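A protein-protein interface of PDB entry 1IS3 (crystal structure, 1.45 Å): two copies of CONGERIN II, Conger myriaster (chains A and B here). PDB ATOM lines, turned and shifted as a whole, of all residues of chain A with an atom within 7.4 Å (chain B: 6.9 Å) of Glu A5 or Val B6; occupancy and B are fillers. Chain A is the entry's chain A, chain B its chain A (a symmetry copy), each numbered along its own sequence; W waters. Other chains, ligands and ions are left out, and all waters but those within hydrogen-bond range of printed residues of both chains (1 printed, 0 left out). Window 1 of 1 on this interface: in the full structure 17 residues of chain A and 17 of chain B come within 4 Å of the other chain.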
ATOM      1  N   ASP A   2       0.972 -17.106 -18.857  1.00  0.00           N
ATOM      2  CA  ASP A   2       0.857 -18.547 -18.903  1.00  0.00           C
ATOM      3  C   ASP A   2      -0.088 -18.761 -17.706  1.00  0.00           C
ATOM      4  O   ASP A   2      -1.044 -17.968 -17.638  1.00  0.00           O
ATOM      5  CB  ASP A   2       2.284 -19.174 -18.743  1.00  0.00           C
ATOM      6  CG  ASP A   2       3.262 -18.459 -17.793  1.00  0.00           C
ATOM      7  OD1 ASP A   2       3.913 -17.502 -18.223  1.00  0.00           O
ATOM      8  OD2 ASP A   2       3.373 -18.846 -16.623  1.00  0.00           O
ATOM      9  N   ARG A   3       0.063 -19.716 -16.770  1.00  0.00           N
ATOM     10  CA  ARG A   3      -0.878 -19.842 -15.668  1.00  0.00           C
ATOM     11  C   ARG A   3      -0.432 -18.881 -14.563  1.00  0.00           C
ATOM     12  O   ARG A   3       0.701 -18.367 -14.537  1.00  0.00           O
ATOM     13  CB  ARG A   3      -0.893 -21.286 -15.183  1.00  0.00           C
ATOM     14  CG  ARG A   3       0.410 -21.723 -14.601  1.00  0.00           C
ATOM     15  CD  ARG A   3       0.401 -23.187 -14.348  1.00  0.00           C
ATOM     16  NE  ARG A   3       1.744 -23.454 -13.946  1.00  0.00           N
ATOM     17  CZ  ARG A   3       2.685 -23.877 -14.804  1.00  0.00           C
ATOM     18  NH1 ARG A   3       3.900 -24.055 -14.309  1.00  0.00           N
ATOM     19  NH2 ARG A   3       2.469 -24.213 -16.081  1.00  0.00           N
ATOM     20  N   ALA A   4      -1.369 -18.673 -13.663  1.00  0.00           N
ATOM     21  CA  ALA A   4      -1.151 -17.780 -12.577  1.00  0.00           C
ATOM     22  C   ALA A   4      -0.601 -18.693 -11.499  1.00  0.00           C
ATOM     23  O   ALA A   4      -1.199 -19.724 -11.170  1.00  0.00           O
ATOM     24  CB  ALA A   4      -2.479 -17.177 -12.184  1.00  0.00           C
ATOM     25  N   GLU A   5       0.541 -18.379 -10.924  1.00  0.00           N
ATOM     26  CA  GLU A   5       1.111 -19.217  -9.870  1.00  0.00           C
ATOM     27  C   GLU A   5       1.869 -18.429  -8.795  1.00  0.00           C
ATOM     28  O   GLU A   5       2.316 -17.285  -9.012  1.00  0.00           O
ATOM     29  CB  GLU A   5       2.023 -20.255 -10.512  1.00  0.00           C
ATOM     30  CG  GLU A   5       3.234 -19.796 -11.259  1.00  0.00           C
ATOM     31  CD  GLU A   5       3.848 -20.858 -12.164  1.00  0.00           C
ATOM     32  OE1 GLU A   5       4.638 -20.462 -13.014  1.00  0.00           O
ATOM     33  OE2 GLU A   5       3.546 -22.052 -12.069  1.00  0.00           O
ATOM     34  N   VAL A   6       1.933 -19.034  -7.606  1.00  0.00           N
ATOM     35  CA  VAL A   6       2.679 -18.487  -6.475  1.00  0.00           C
ATOM     36  C   VAL A   6       3.615 -19.665  -6.209  1.00  0.00           C
ATOM     37  O   VAL A   6       3.139 -20.774  -5.916  1.00  0.00           O
ATOM     38  CB  VAL A   6       1.740 -18.218  -5.265  1.00  0.00           C
ATOM     39  CG1 VAL A   6       2.613 -17.721  -4.109  1.00  0.00           C
ATOM     40  CG2 VAL A   6       0.629 -17.202  -5.606  1.00  0.00           C
ATOM     41  N   ARG A   7       4.918 -19.484  -6.308  1.00  0.00           N
ATOM     42  CA  ARG A   7       5.883 -20.559  -6.242  1.00  0.00           C
ATOM     43  C   ARG A   7       6.965 -20.211  -5.238  1.00  0.00           C
ATOM     44  O   ARG A   7       7.492 -19.097  -5.192  1.00  0.00           O
ATOM     45  CB  ARG A   7       6.487 -20.748  -7.639  1.00  0.00           C
ATOM     46  CG  ARG A   7       7.545 -21.822  -7.710  1.00  0.00           C
ATOM     47  CD  ARG A   7       8.135 -21.798  -9.128  1.00  0.00           C
ATOM     48  NE  ARG A   7       7.169 -22.190 -10.157  1.00  0.00           N
ATOM     49  CZ  ARG A   7       6.935 -23.489 -10.467  1.00  0.00           C
ATOM     50  NH1 ARG A   7       7.585 -24.486  -9.837  1.00  0.00           N
ATOM     51  NH2 ARG A   7       6.019 -23.826 -11.400  1.00  0.00           N
ATOM     52  N   ILE A   9       6.884 -19.869  -1.996  1.00  0.00           N
ATOM     53  CA  ILE A   9       6.545 -19.146  -0.814  1.00  0.00           C
ATOM     54  C   ILE A   9       5.717 -20.212  -0.082  1.00  0.00           C
ATOM     55  O   ILE A   9       4.533 -20.423  -0.406  1.00  0.00           O
ATOM     56  CB  ILE A   9       5.714 -17.877  -1.142  1.00  0.00           C
ATOM     57  CG1 ILE A   9       6.494 -16.980  -2.128  1.00  0.00           C
ATOM     58  CG2 ILE A   9       5.393 -17.160   0.177  1.00  0.00           C
ATOM     59  CD1 ILE A   9       5.721 -15.773  -2.690  1.00  0.00           C
ATOM     60  N   THR A  38       3.195 -29.182 -11.400  1.00  0.00           N
ATOM     61  CA  THR A  38       2.008 -29.449 -12.189  1.00  0.00           C
ATOM     62  C   THR A  38       1.730 -30.949 -12.344  1.00  0.00           C
ATOM     63  O   THR A  38       0.729 -31.291 -13.000  1.00  0.00           O
ATOM     64  CB  THR A  38       2.134 -28.767 -13.603  1.00  0.00           C
ATOM     65  OG1 THR A  38       3.252 -29.384 -14.218  1.00  0.00           O
ATOM     66  CG2 THR A  38       2.217 -27.217 -13.558  1.00  0.00           C
ATOM     67  N   LEU A 120       3.735 -24.816  -4.262  1.00  0.00           N
ATOM     68  CA  LEU A 120       3.162 -24.319  -5.505  1.00  0.00           C
ATOM     69  C   LEU A 120       1.638 -24.182  -5.385  1.00  0.00           C
ATOM     70  O   LEU A 120       0.960 -25.119  -4.938  1.00  0.00           O
ATOM     71  CB  LEU A 120       3.492 -25.276  -6.668  1.00  0.00           C
ATOM     72  CG  LEU A 120       2.902 -24.903  -8.041  1.00  0.00           C
ATOM     73  CD1 LEU A 120       3.528 -23.598  -8.503  1.00  0.00           C
ATOM     74  CD2 LEU A 120       3.175 -25.969  -9.071  1.00  0.00           C
ATOM     75  N   ILE A 121       1.108 -23.023  -5.731  1.00  0.00           N
ATOM     76  CA  ILE A 121      -0.314 -22.786  -5.776  1.00  0.00           C
ATOM     77  C   ILE A 121      -0.540 -22.281  -7.193  1.00  0.00           C
ATOM     78  O   ILE A 121       0.190 -21.365  -7.595  1.00  0.00           O
ATOM     79  CB  ILE A 121      -0.688 -21.722  -4.736  1.00  0.00           C
ATOM     80  CG1 ILE A 121      -0.465 -22.242  -3.336  1.00  0.00           C
ATOM     81  CG2 ILE A 121      -2.132 -21.330  -4.933  1.00  0.00           C
ATOM     82  CD1 ILE A 121       0.258 -21.166  -2.513  1.00  0.00           C
ATOM     83  N   TYR A 122      -1.455 -22.803  -8.018  1.00  0.00           N
ATOM     84  CA  TYR A 122      -1.679 -22.223  -9.317  1.00  0.00           C
ATOM     85  C   TYR A 122      -3.114 -22.421  -9.758  1.00  0.00           C
ATOM     86  O   TYR A 122      -3.820 -23.333  -9.289  1.00  0.00           O
ATOM     87  CB  TYR A 122      -0.757 -22.824 -10.382  1.00  0.00           C
ATOM     88  CG  TYR A 122      -0.973 -24.268 -10.836  1.00  0.00           C
ATOM     89  CD1 TYR A 122      -1.721 -24.533 -11.988  1.00  0.00           C
ATOM     90  CD2 TYR A 122      -0.341 -25.312 -10.175  1.00  0.00           C
ATOM     91  CE1 TYR A 122      -1.816 -25.830 -12.489  1.00  0.00           C
ATOM     92  CE2 TYR A 122      -0.439 -26.621 -10.679  1.00  0.00           C
ATOM     93  CZ  TYR A 122      -1.175 -26.879 -11.841  1.00  0.00           C
ATOM     94  OH  TYR A 122      -1.234 -28.178 -12.358  1.00  0.00           O
ATOM     95  N   LEU A 123      -3.513 -21.557 -10.675  1.00  0.00           N
ATOM     96  CA  LEU A 123      -4.830 -21.628 -11.297  1.00  0.00           C
ATOM     97  C   LEU A 123      -4.594 -22.048 -12.730  1.00  0.00           C
ATOM     98  O   LEU A 123      -3.662 -21.542 -13.378  1.00  0.00           O
ATOM     99  CB  LEU A 123      -5.532 -20.250 -11.265  1.00  0.00           C
ATOM    100  CG  LEU A 123      -6.935 -20.192 -11.877  1.00  0.00           C
ATOM    101  CD1 LEU A 123      -7.968 -19.595 -10.926  1.00  0.00           C
ATOM    102  CD2 LEU A 123      -6.816 -19.379 -13.142  1.00  0.00           C
ATOM    103  N   LEU A 129      -6.734 -14.837 -12.102  1.00  0.00           N
ATOM    104  CA  LEU A 129      -6.683 -14.366 -10.724  1.00  0.00           C
ATOM    105  C   LEU A 129      -6.428 -12.862 -10.708  1.00  0.00           C
ATOM    106  O   LEU A 129      -5.777 -12.320 -11.602  1.00  0.00           O
ATOM    107  CB  LEU A 129      -5.562 -15.069  -9.907  1.00  0.00           C
ATOM    108  CG  LEU A 129      -5.696 -16.568  -9.561  1.00  0.00           C
ATOM    109  CD1 LEU A 129      -4.504 -17.088  -8.748  1.00  0.00           C
ATOM    110  CD2 LEU A 129      -7.024 -16.743  -8.796  1.00  0.00           C
ATOM    111  N   VAL A 132      -4.198 -12.097  -4.333  1.00  0.00           N
ATOM    112  CA  VAL A 132      -3.809 -13.233  -3.526  1.00  0.00           C
ATOM    113  C   VAL A 132      -3.309 -12.742  -2.163  1.00  0.00           C
ATOM    114  O   VAL A 132      -2.595 -11.719  -2.088  1.00  0.00           O
ATOM    115  CB  VAL A 132      -2.690 -14.064  -4.271  1.00  0.00           C
ATOM    116  CG1 VAL A 132      -1.386 -13.239  -4.508  1.00  0.00           C
ATOM    117  CG2 VAL A 132      -2.375 -15.303  -3.424  1.00  0.00           C
ATOM    118  N   ALA B   4      11.466 -17.482  -5.444  1.00  0.00           N
ATOM    119  CA  ALA B   4      10.140 -17.318  -4.954  1.00  0.00           C
ATOM    120  C   ALA B   4       9.532 -16.350  -5.950  1.00  0.00           C
ATOM    121  O   ALA B   4      10.087 -15.278  -6.219  1.00  0.00           O
ATOM    122  CB  ALA B   4      10.217 -16.728  -3.566  1.00  0.00           C
ATOM    123  N   GLU B   5       8.402 -16.675  -6.542  1.00  0.00           N
ATOM    124  CA  GLU B   5       7.765 -15.774  -7.501  1.00  0.00           C
ATOM    125  C   GLU B   5       6.233 -15.824  -7.474  1.00  0.00           C
ATOM    126  O   GLU B   5       5.617 -16.806  -7.015  1.00  0.00           O
ATOM    127  CB  GLU B   5       8.284 -16.100  -8.896  1.00  0.00           C
ATOM    128  CG  GLU B   5       8.007 -17.450  -9.478  1.00  0.00           C
ATOM    129  CD  GLU B   5       8.874 -17.799 -10.681  1.00  0.00           C
ATOM    130  OE1 GLU B   5       8.909 -18.982 -11.004  1.00  0.00           O
ATOM    131  OE2 GLU B   5       9.533 -16.946 -11.283  1.00  0.00           O
ATOM    132  N   VAL B   6       5.635 -14.710  -7.902  1.00  0.00           N
ATOM    133  CA  VAL B   6       4.185 -14.585  -8.031  1.00  0.00           C
ATOM    134  C   VAL B   6       4.102 -14.221  -9.512  1.00  0.00           C
ATOM    135  O   VAL B   6       4.662 -13.192  -9.925  1.00  0.00           O
ATOM    136  CB  VAL B   6       3.640 -13.440  -7.130  1.00  0.00           C
ATOM    137  CG1 VAL B   6       2.134 -13.333  -7.384  1.00  0.00           C
ATOM    138  CG2 VAL B   6       3.941 -13.684  -5.636  1.00  0.00           C
ATOM    139  N   ARG B   7       3.446 -15.018 -10.334  1.00  0.00           N
ATOM    140  CA  ARG B   7       3.444 -14.863 -11.771  1.00  0.00           C
ATOM    141  C   ARG B   7       2.017 -14.880 -12.284  1.00  0.00           C
ATOM    142  O   ARG B   7       1.185 -15.704 -11.895  1.00  0.00           O
ATOM    143  CB  ARG B   7       4.250 -16.016 -12.380  1.00  0.00           C
ATOM    144  CG  ARG B   7       4.302 -16.000 -13.888  1.00  0.00           C
ATOM    145  CD  ARG B   7       5.026 -17.277 -14.341  1.00  0.00           C
ATOM    146  NE  ARG B   7       6.435 -17.308 -13.943  1.00  0.00           N
ATOM    147  CZ  ARG B   7       7.404 -16.710 -14.679  1.00  0.00           C
ATOM    148  NH1 ARG B   7       7.111 -16.054 -15.818  1.00  0.00           N
ATOM    149  NH2 ARG B   7       8.692 -16.728 -14.276  1.00  0.00           N
ATOM    150  N   ASN B   8       1.758 -13.923 -13.161  1.00  0.00           N
ATOM    151  CA  ASN B   8       0.493 -13.753 -13.880  1.00  0.00           C
ATOM    152  C   ASN B   8      -0.713 -13.447 -13.009  1.00  0.00           C
ATOM    153  O   ASN B   8      -1.870 -13.732 -13.338  1.00  0.00           O
ATOM    154  CB  ASN B   8       0.218 -15.008 -14.784  1.00  0.00           C
ATOM    155  CG  ASN B   8       1.246 -15.131 -15.914  1.00  0.00           C
ATOM    156  OD1 ASN B   8       1.700 -16.196 -16.356  1.00  0.00           O
ATOM    157  ND2 ASN B   8       1.637 -14.036 -16.540  1.00  0.00           N
ATOM    158  N   ILE B   9      -0.454 -12.790 -11.892  1.00  0.00           N
ATOM    159  CA  ILE B   9      -1.493 -12.200 -11.114  1.00  0.00           C
ATOM    160  C   ILE B   9      -1.098 -10.720 -11.228  1.00  0.00           C
ATOM    161  O   ILE B   9      -0.179 -10.256 -10.527  1.00  0.00           O
ATOM    162  CB  ILE B   9      -1.461 -12.705  -9.647  1.00  0.00           C
ATOM    163  CG1 ILE B   9      -1.567 -14.247  -9.622  1.00  0.00           C
ATOM    164  CG2 ILE B   9      -2.605 -12.026  -8.881  1.00  0.00           C
ATOM    165  CD1 ILE B   9      -1.364 -14.908  -8.247  1.00  0.00           C
ATOM    166  N   LEU B  17       1.454  -4.329  -2.813  1.00  0.00           N
ATOM    167  CA  LEU B  17       2.182  -5.584  -2.681  1.00  0.00           C
ATOM    168  C   LEU B  17       2.912  -5.548  -1.343  1.00  0.00           C
ATOM    169  O   LEU B  17       3.751  -4.633  -1.134  1.00  0.00           O
ATOM    170  CB  LEU B  17       3.226  -5.721  -3.778  1.00  0.00           C
ATOM    171  CG  LEU B  17       4.257  -6.856  -3.649  1.00  0.00           C
ATOM    172  CD1 LEU B  17       3.525  -8.205  -3.720  1.00  0.00           C
ATOM    173  CD2 LEU B  17       5.350  -6.714  -4.722  1.00  0.00           C
ATOM    174  N   VAL B  19       5.375  -8.032   0.969  1.00  0.00           N
ATOM    175  CA  VAL B  19       6.085  -9.301   1.073  1.00  0.00           C
ATOM    176  C   VAL B  19       6.829  -9.324   2.397  1.00  0.00           C
ATOM    177  O   VAL B  19       7.251  -8.273   2.899  1.00  0.00           O
ATOM    178  CB  VAL B  19       7.130  -9.538  -0.062  1.00  0.00           C
ATOM    179  CG1 VAL B  19       6.394  -9.811  -1.376  1.00  0.00           C
ATOM    180  CG2 VAL B  19       8.043  -8.325  -0.245  1.00  0.00           C
ATOM    181  N   PHE B 118       2.232  -5.171 -13.955  1.00  0.00           N
ATOM    182  CA  PHE B 118       3.421  -6.027 -14.035  1.00  0.00           C
ATOM    183  C   PHE B 118       2.959  -7.446 -13.785  1.00  0.00           C
ATOM    184  O   PHE B 118       2.150  -7.655 -12.868  1.00  0.00           O
ATOM    185  CB  PHE B 118       4.461  -5.673 -12.955  1.00  0.00           C
ATOM    186  CG  PHE B 118       4.943  -4.250 -13.118  1.00  0.00           C
ATOM    187  CD1 PHE B 118       5.828  -3.927 -14.167  1.00  0.00           C
ATOM    188  CD2 PHE B 118       4.451  -3.254 -12.273  1.00  0.00           C
ATOM    189  CE1 PHE B 118       6.194  -2.591 -14.360  1.00  0.00           C
ATOM    190  CE2 PHE B 118       4.832  -1.919 -12.479  1.00  0.00           C
ATOM    191  CZ  PHE B 118       5.691  -1.599 -13.517  1.00  0.00           C
ATOM    192  N   ASN B 119       3.479  -8.393 -14.567  1.00  0.00           N
ATOM    193  CA  ASN B 119       3.076  -9.770 -14.376  1.00  0.00           C
ATOM    194  C   ASN B 119       4.040 -10.687 -13.647  1.00  0.00           C
ATOM    195  O   ASN B 119       3.775 -11.906 -13.548  1.00  0.00           O
ATOM    196  CB  ASN B 119       2.718 -10.379 -15.733  1.00  0.00           C
ATOM    197  CG  ASN B 119       1.244 -10.101 -16.064  1.00  0.00           C
ATOM    198  OD1 ASN B 119       0.549  -9.240 -15.520  1.00  0.00           O
ATOM    199  ND2 ASN B 119       0.675 -10.793 -17.033  1.00  0.00           N
ATOM    200  N   LEU B 120       5.131 -10.165 -13.094  1.00  0.00           N
ATOM    201  CA  LEU B 120       6.071 -11.013 -12.374  1.00  0.00           C
ATOM    202  C   LEU B 120       6.668 -10.264 -11.174  1.00  0.00           C
ATOM    203  O   LEU B 120       7.132  -9.124 -11.315  1.00  0.00           O
ATOM    204  CB  LEU B 120       7.214 -11.459 -13.307  1.00  0.00           C
ATOM    205  CG  LEU B 120       8.317 -12.321 -12.664  1.00  0.00           C
ATOM    206  CD1 LEU B 120       7.711 -13.646 -12.231  1.00  0.00           C
ATOM    207  CD2 LEU B 120       9.444 -12.591 -13.628  1.00  0.00           C
ATOM    208  N   ILE B 121       6.617 -10.870 -10.001  1.00  0.00           N
ATOM    209  CA  ILE B 121       7.234 -10.339  -8.810  1.00  0.00           C
ATOM    210  C   ILE B 121       8.125 -11.479  -8.341  1.00  0.00           C
ATOM    211  O   ILE B 121       7.613 -12.602  -8.248  1.00  0.00           O
ATOM    212  CB  ILE B 121       6.150 -10.014  -7.775  1.00  0.00           C
ATOM    213  CG1 ILE B 121       5.280  -8.877  -8.252  1.00  0.00           C
ATOM    214  CG2 ILE B 121       6.812  -9.660  -6.465  1.00  0.00           C
ATOM    215  CD1 ILE B 121       3.807  -9.238  -8.009  1.00  0.00           C
ATOM    216  N   TYR B 122       9.425 -11.324  -8.063  1.00  0.00           N
ATOM    217  CA  TYR B 122      10.194 -12.423  -7.540  1.00  0.00           C
ATOM    218  C   TYR B 122      11.315 -11.926  -6.651  1.00  0.00           C
ATOM    219  O   TYR B 122      11.765 -10.770  -6.755  1.00  0.00           O
ATOM    220  CB  TYR B 122      10.802 -13.281  -8.653  1.00  0.00           C
ATOM    221  CG  TYR B 122      11.937 -12.714  -9.506  1.00  0.00           C
ATOM    222  CD1 TYR B 122      13.266 -13.003  -9.182  1.00  0.00           C
ATOM    223  CD2 TYR B 122      11.653 -12.002 -10.664  1.00  0.00           C
ATOM    224  CE1 TYR B 122      14.304 -12.605 -10.023  1.00  0.00           C
ATOM    225  CE2 TYR B 122      12.701 -11.598 -11.510  1.00  0.00           C
ATOM    226  CZ  TYR B 122      14.029 -11.903 -11.191  1.00  0.00           C
ATOM    227  OH  TYR B 122      15.061 -11.533 -12.060  1.00  0.00           O
ATOM    228  N   LEU B 123      11.755 -12.830  -5.794  1.00  0.00           N
ATOM    229  CA  LEU B 123      12.888 -12.582  -4.908  1.00  0.00           C
ATOM    230  C   LEU B 123      14.012 -13.459  -5.412  1.00  0.00           C
ATOM    231  O   LEU B 123      13.777 -14.629  -5.756  1.00  0.00           O
ATOM    232  CB  LEU B 123      12.542 -12.961  -3.449  1.00  0.00           C
ATOM    233  CG  LEU B 123      13.647 -12.735  -2.412  1.00  0.00           C
ATOM    234  CD1 LEU B 123      13.178 -11.899  -1.225  1.00  0.00           C
ATOM    235  CD2 LEU B 123      14.109 -14.103  -1.976  1.00  0.00           C
ATOM    236  N   LEU B 129      11.116 -15.869   1.129  1.00  0.00           N
ATOM    237  CA  LEU B 129       9.865 -15.196   1.458  1.00  0.00           C
ATOM    238  C   LEU B 129       9.000 -16.118   2.312  1.00  0.00           C
ATOM    239  O   LEU B 129       9.064 -17.342   2.188  1.00  0.00           O
ATOM    240  CB  LEU B 129       9.063 -14.798   0.187  1.00  0.00           C
ATOM    241  CG  LEU B 129       9.606 -13.688  -0.741  1.00  0.00           C
ATOM    242  CD1 LEU B 129       8.683 -13.424  -1.937  1.00  0.00           C
ATOM    243  CD2 LEU B 129       9.790 -12.423   0.123  1.00  0.00           C
ATOM    244  N   VAL B 132       2.920 -13.213   1.416  1.00  0.00           N
ATOM    245  CA  VAL B 132       2.696 -12.234   0.375  1.00  0.00           C
ATOM    246  C   VAL B 132       1.226 -11.800   0.392  1.00  0.00           C
ATOM    247  O   VAL B 132       0.325 -12.644   0.583  1.00  0.00           O
ATOM    248  CB  VAL B 132       3.088 -12.843  -1.030  1.00  0.00           C
ATOM    249  CG1 VAL B 132       2.217 -14.082  -1.412  1.00  0.00           C
ATOM    250  CG2 VAL B 132       2.920 -11.745  -2.088  1.00  0.00           C
ATOM    251  N   LEU B 134      -1.080  -9.344  -2.268  1.00  0.00           N
ATOM    252  CA  LEU B 134      -1.120  -8.533  -3.482  1.00  0.00           C
ATOM    253  C   LEU B 134      -2.602  -8.279  -3.730  1.00  0.00           C
ATOM    254  O   LEU B 134      -3.338  -9.209  -4.114  1.00  0.00           O
ATOM    255  CB  LEU B 134      -0.514  -9.293  -4.666  1.00  0.00           C
ATOM    256  CG  LEU B 134      -0.646  -8.616  -6.050  1.00  0.00           C
ATOM    257  CD1 LEU B 134       0.041  -7.249  -5.963  1.00  0.00           C
ATOM    258  CD2 LEU B 134      -0.057  -9.500  -7.149  1.00  0.00           C
HETATM  259  O   HOH W   1      -4.508 -14.704 -13.794  1.00  0.00           O
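OD1 of Asn B8 is in hydrogen-bond range of N of Asp A2 (2.8 Å).
The backbone carbonyl oxygen (O) of Arg A3 lies close to the side-chain amide oxygen (OD1) of Asn B8 (3.0 Å).
OE1 of Glu A5 is in salt-bridge range of NE of Arg B7 (3.7 Å).
NE of Arg A7 lies within salt-bridge range of OE1 of Glu B5 (3.7 Å).
O of Val A132 is in hydrogen-bond range of N of Leu B134 (2.8 Å).
The backbone carbonyl oxygen of Ala A4 is in hydrogen-bond range of the backbone NH of Leu A123, 3.0 Å away.
The side-chain carboxylate (OE2) of Glu A5 is in salt-bridge range of the guanidinium group (NH2) of Arg A7 (3.1 Å).
The backbone NH (N) of Val A6 lies within hydrogen-bond range of the backbone carbonyl oxygen (O) of Ile A121, at 2.9 Å.
The backbone carbonyl oxygen (O) of Ala B4 sits at hydrogen-bond distance from the backbone NH (N) of Leu B123 (3.0 Å).
OE2 of Glu B5 is in salt-bridge range of NH2 of Arg B7 (3.1 Å).
O of Ile B121 is in hydrogen-bond range of N of Val B6, 2.9 Å away.
Asp A2 touches Arg B7.
Arg B7 touches Arg A3 (O to O, 3.8 Å).
CB of Ala A4 touches O of Asn B8, 3.7 Å away.
Ile B9 touches Ala A4 (CG1 to CB, 3.998 Å).
O of Glu A5 touches O of Glu B5, 3.9 Å away.
O of Glu A5 touches CA of Val B6, at 3.4 Å.
Ala B4 touches Arg A7.
CB of Ala B4 touches CG1 of Ile A9 (3.999 Å).
Leu B129 touches Ile A9.
CD1 of Leu A129 touches CD1 of Ile B9 (3.9 Å).
Of the printed residues of chain B, Arg A3 touches Arg B7 and Asn B8.
Printed residues of chain B within 4 Å of Ala A4: Arg B7 (3.2 Å), Asn B8 (3.7 Å) and Ile B9 (3.998 Å).
Glu A5 touches three residues of chain B.
Printed residues of chain A within 4 Å of Glu B5: Glu A5 (3.9 Å), Val A6 (3.4 Å) and Arg A7 (2.9 Å).
Of chain A, only Glu A5 comes within 4 Å of Val B6.
Of the printed residues of chain A, Ile B9 touches Ala A4 and Leu A129.
Of the printed residues of chain A, Leu B129 touches Ile A9.
The nearest residue of chain B that does not touch Glu A5 is Ile B9 (4.4 Å).
The nearest printed residue of chain B that does not touch Val A132 is Val B132 (4.1 Å).
Of the 14 printed residues of chain A, 9 touch a printed residue of chain B.
Hydrophobic or aromatic side chains of chain A within 4 Å of the printed part of chain B: Ala A4, Ile A9 and Leu A129.
Along chain A the printed residues that touch a printed residue of chain B span positions 2 to 132.
Among the printed residues, 17 pairs touch across the chains.
Ala A4 touches Arg B7, and with the chains exchanged Arg A7 touches Ala B4.
Ala A4 touches Ile B9, and with the chains exchanged Ile A9 touches Ala B4.
Glu A5 touches its own counterpart, Glu B5.
Glu A5 touches Arg B7, and with the chains exchanged Arg A7 touches Glu B5.
Positions printed for both chains: 4, 5, 6, 7, 9, 120, 121, 122, 123, 129 and 132.
Of the 17 pairs that touch across the chains among the printed residues, 11 have their exchanged pair printed and touching as well.
Water W1 lies within hydrogen-bond range of the backbone NH (N) of Leu A129 and the backbone carbonyl oxygen (O) of Asn B8.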
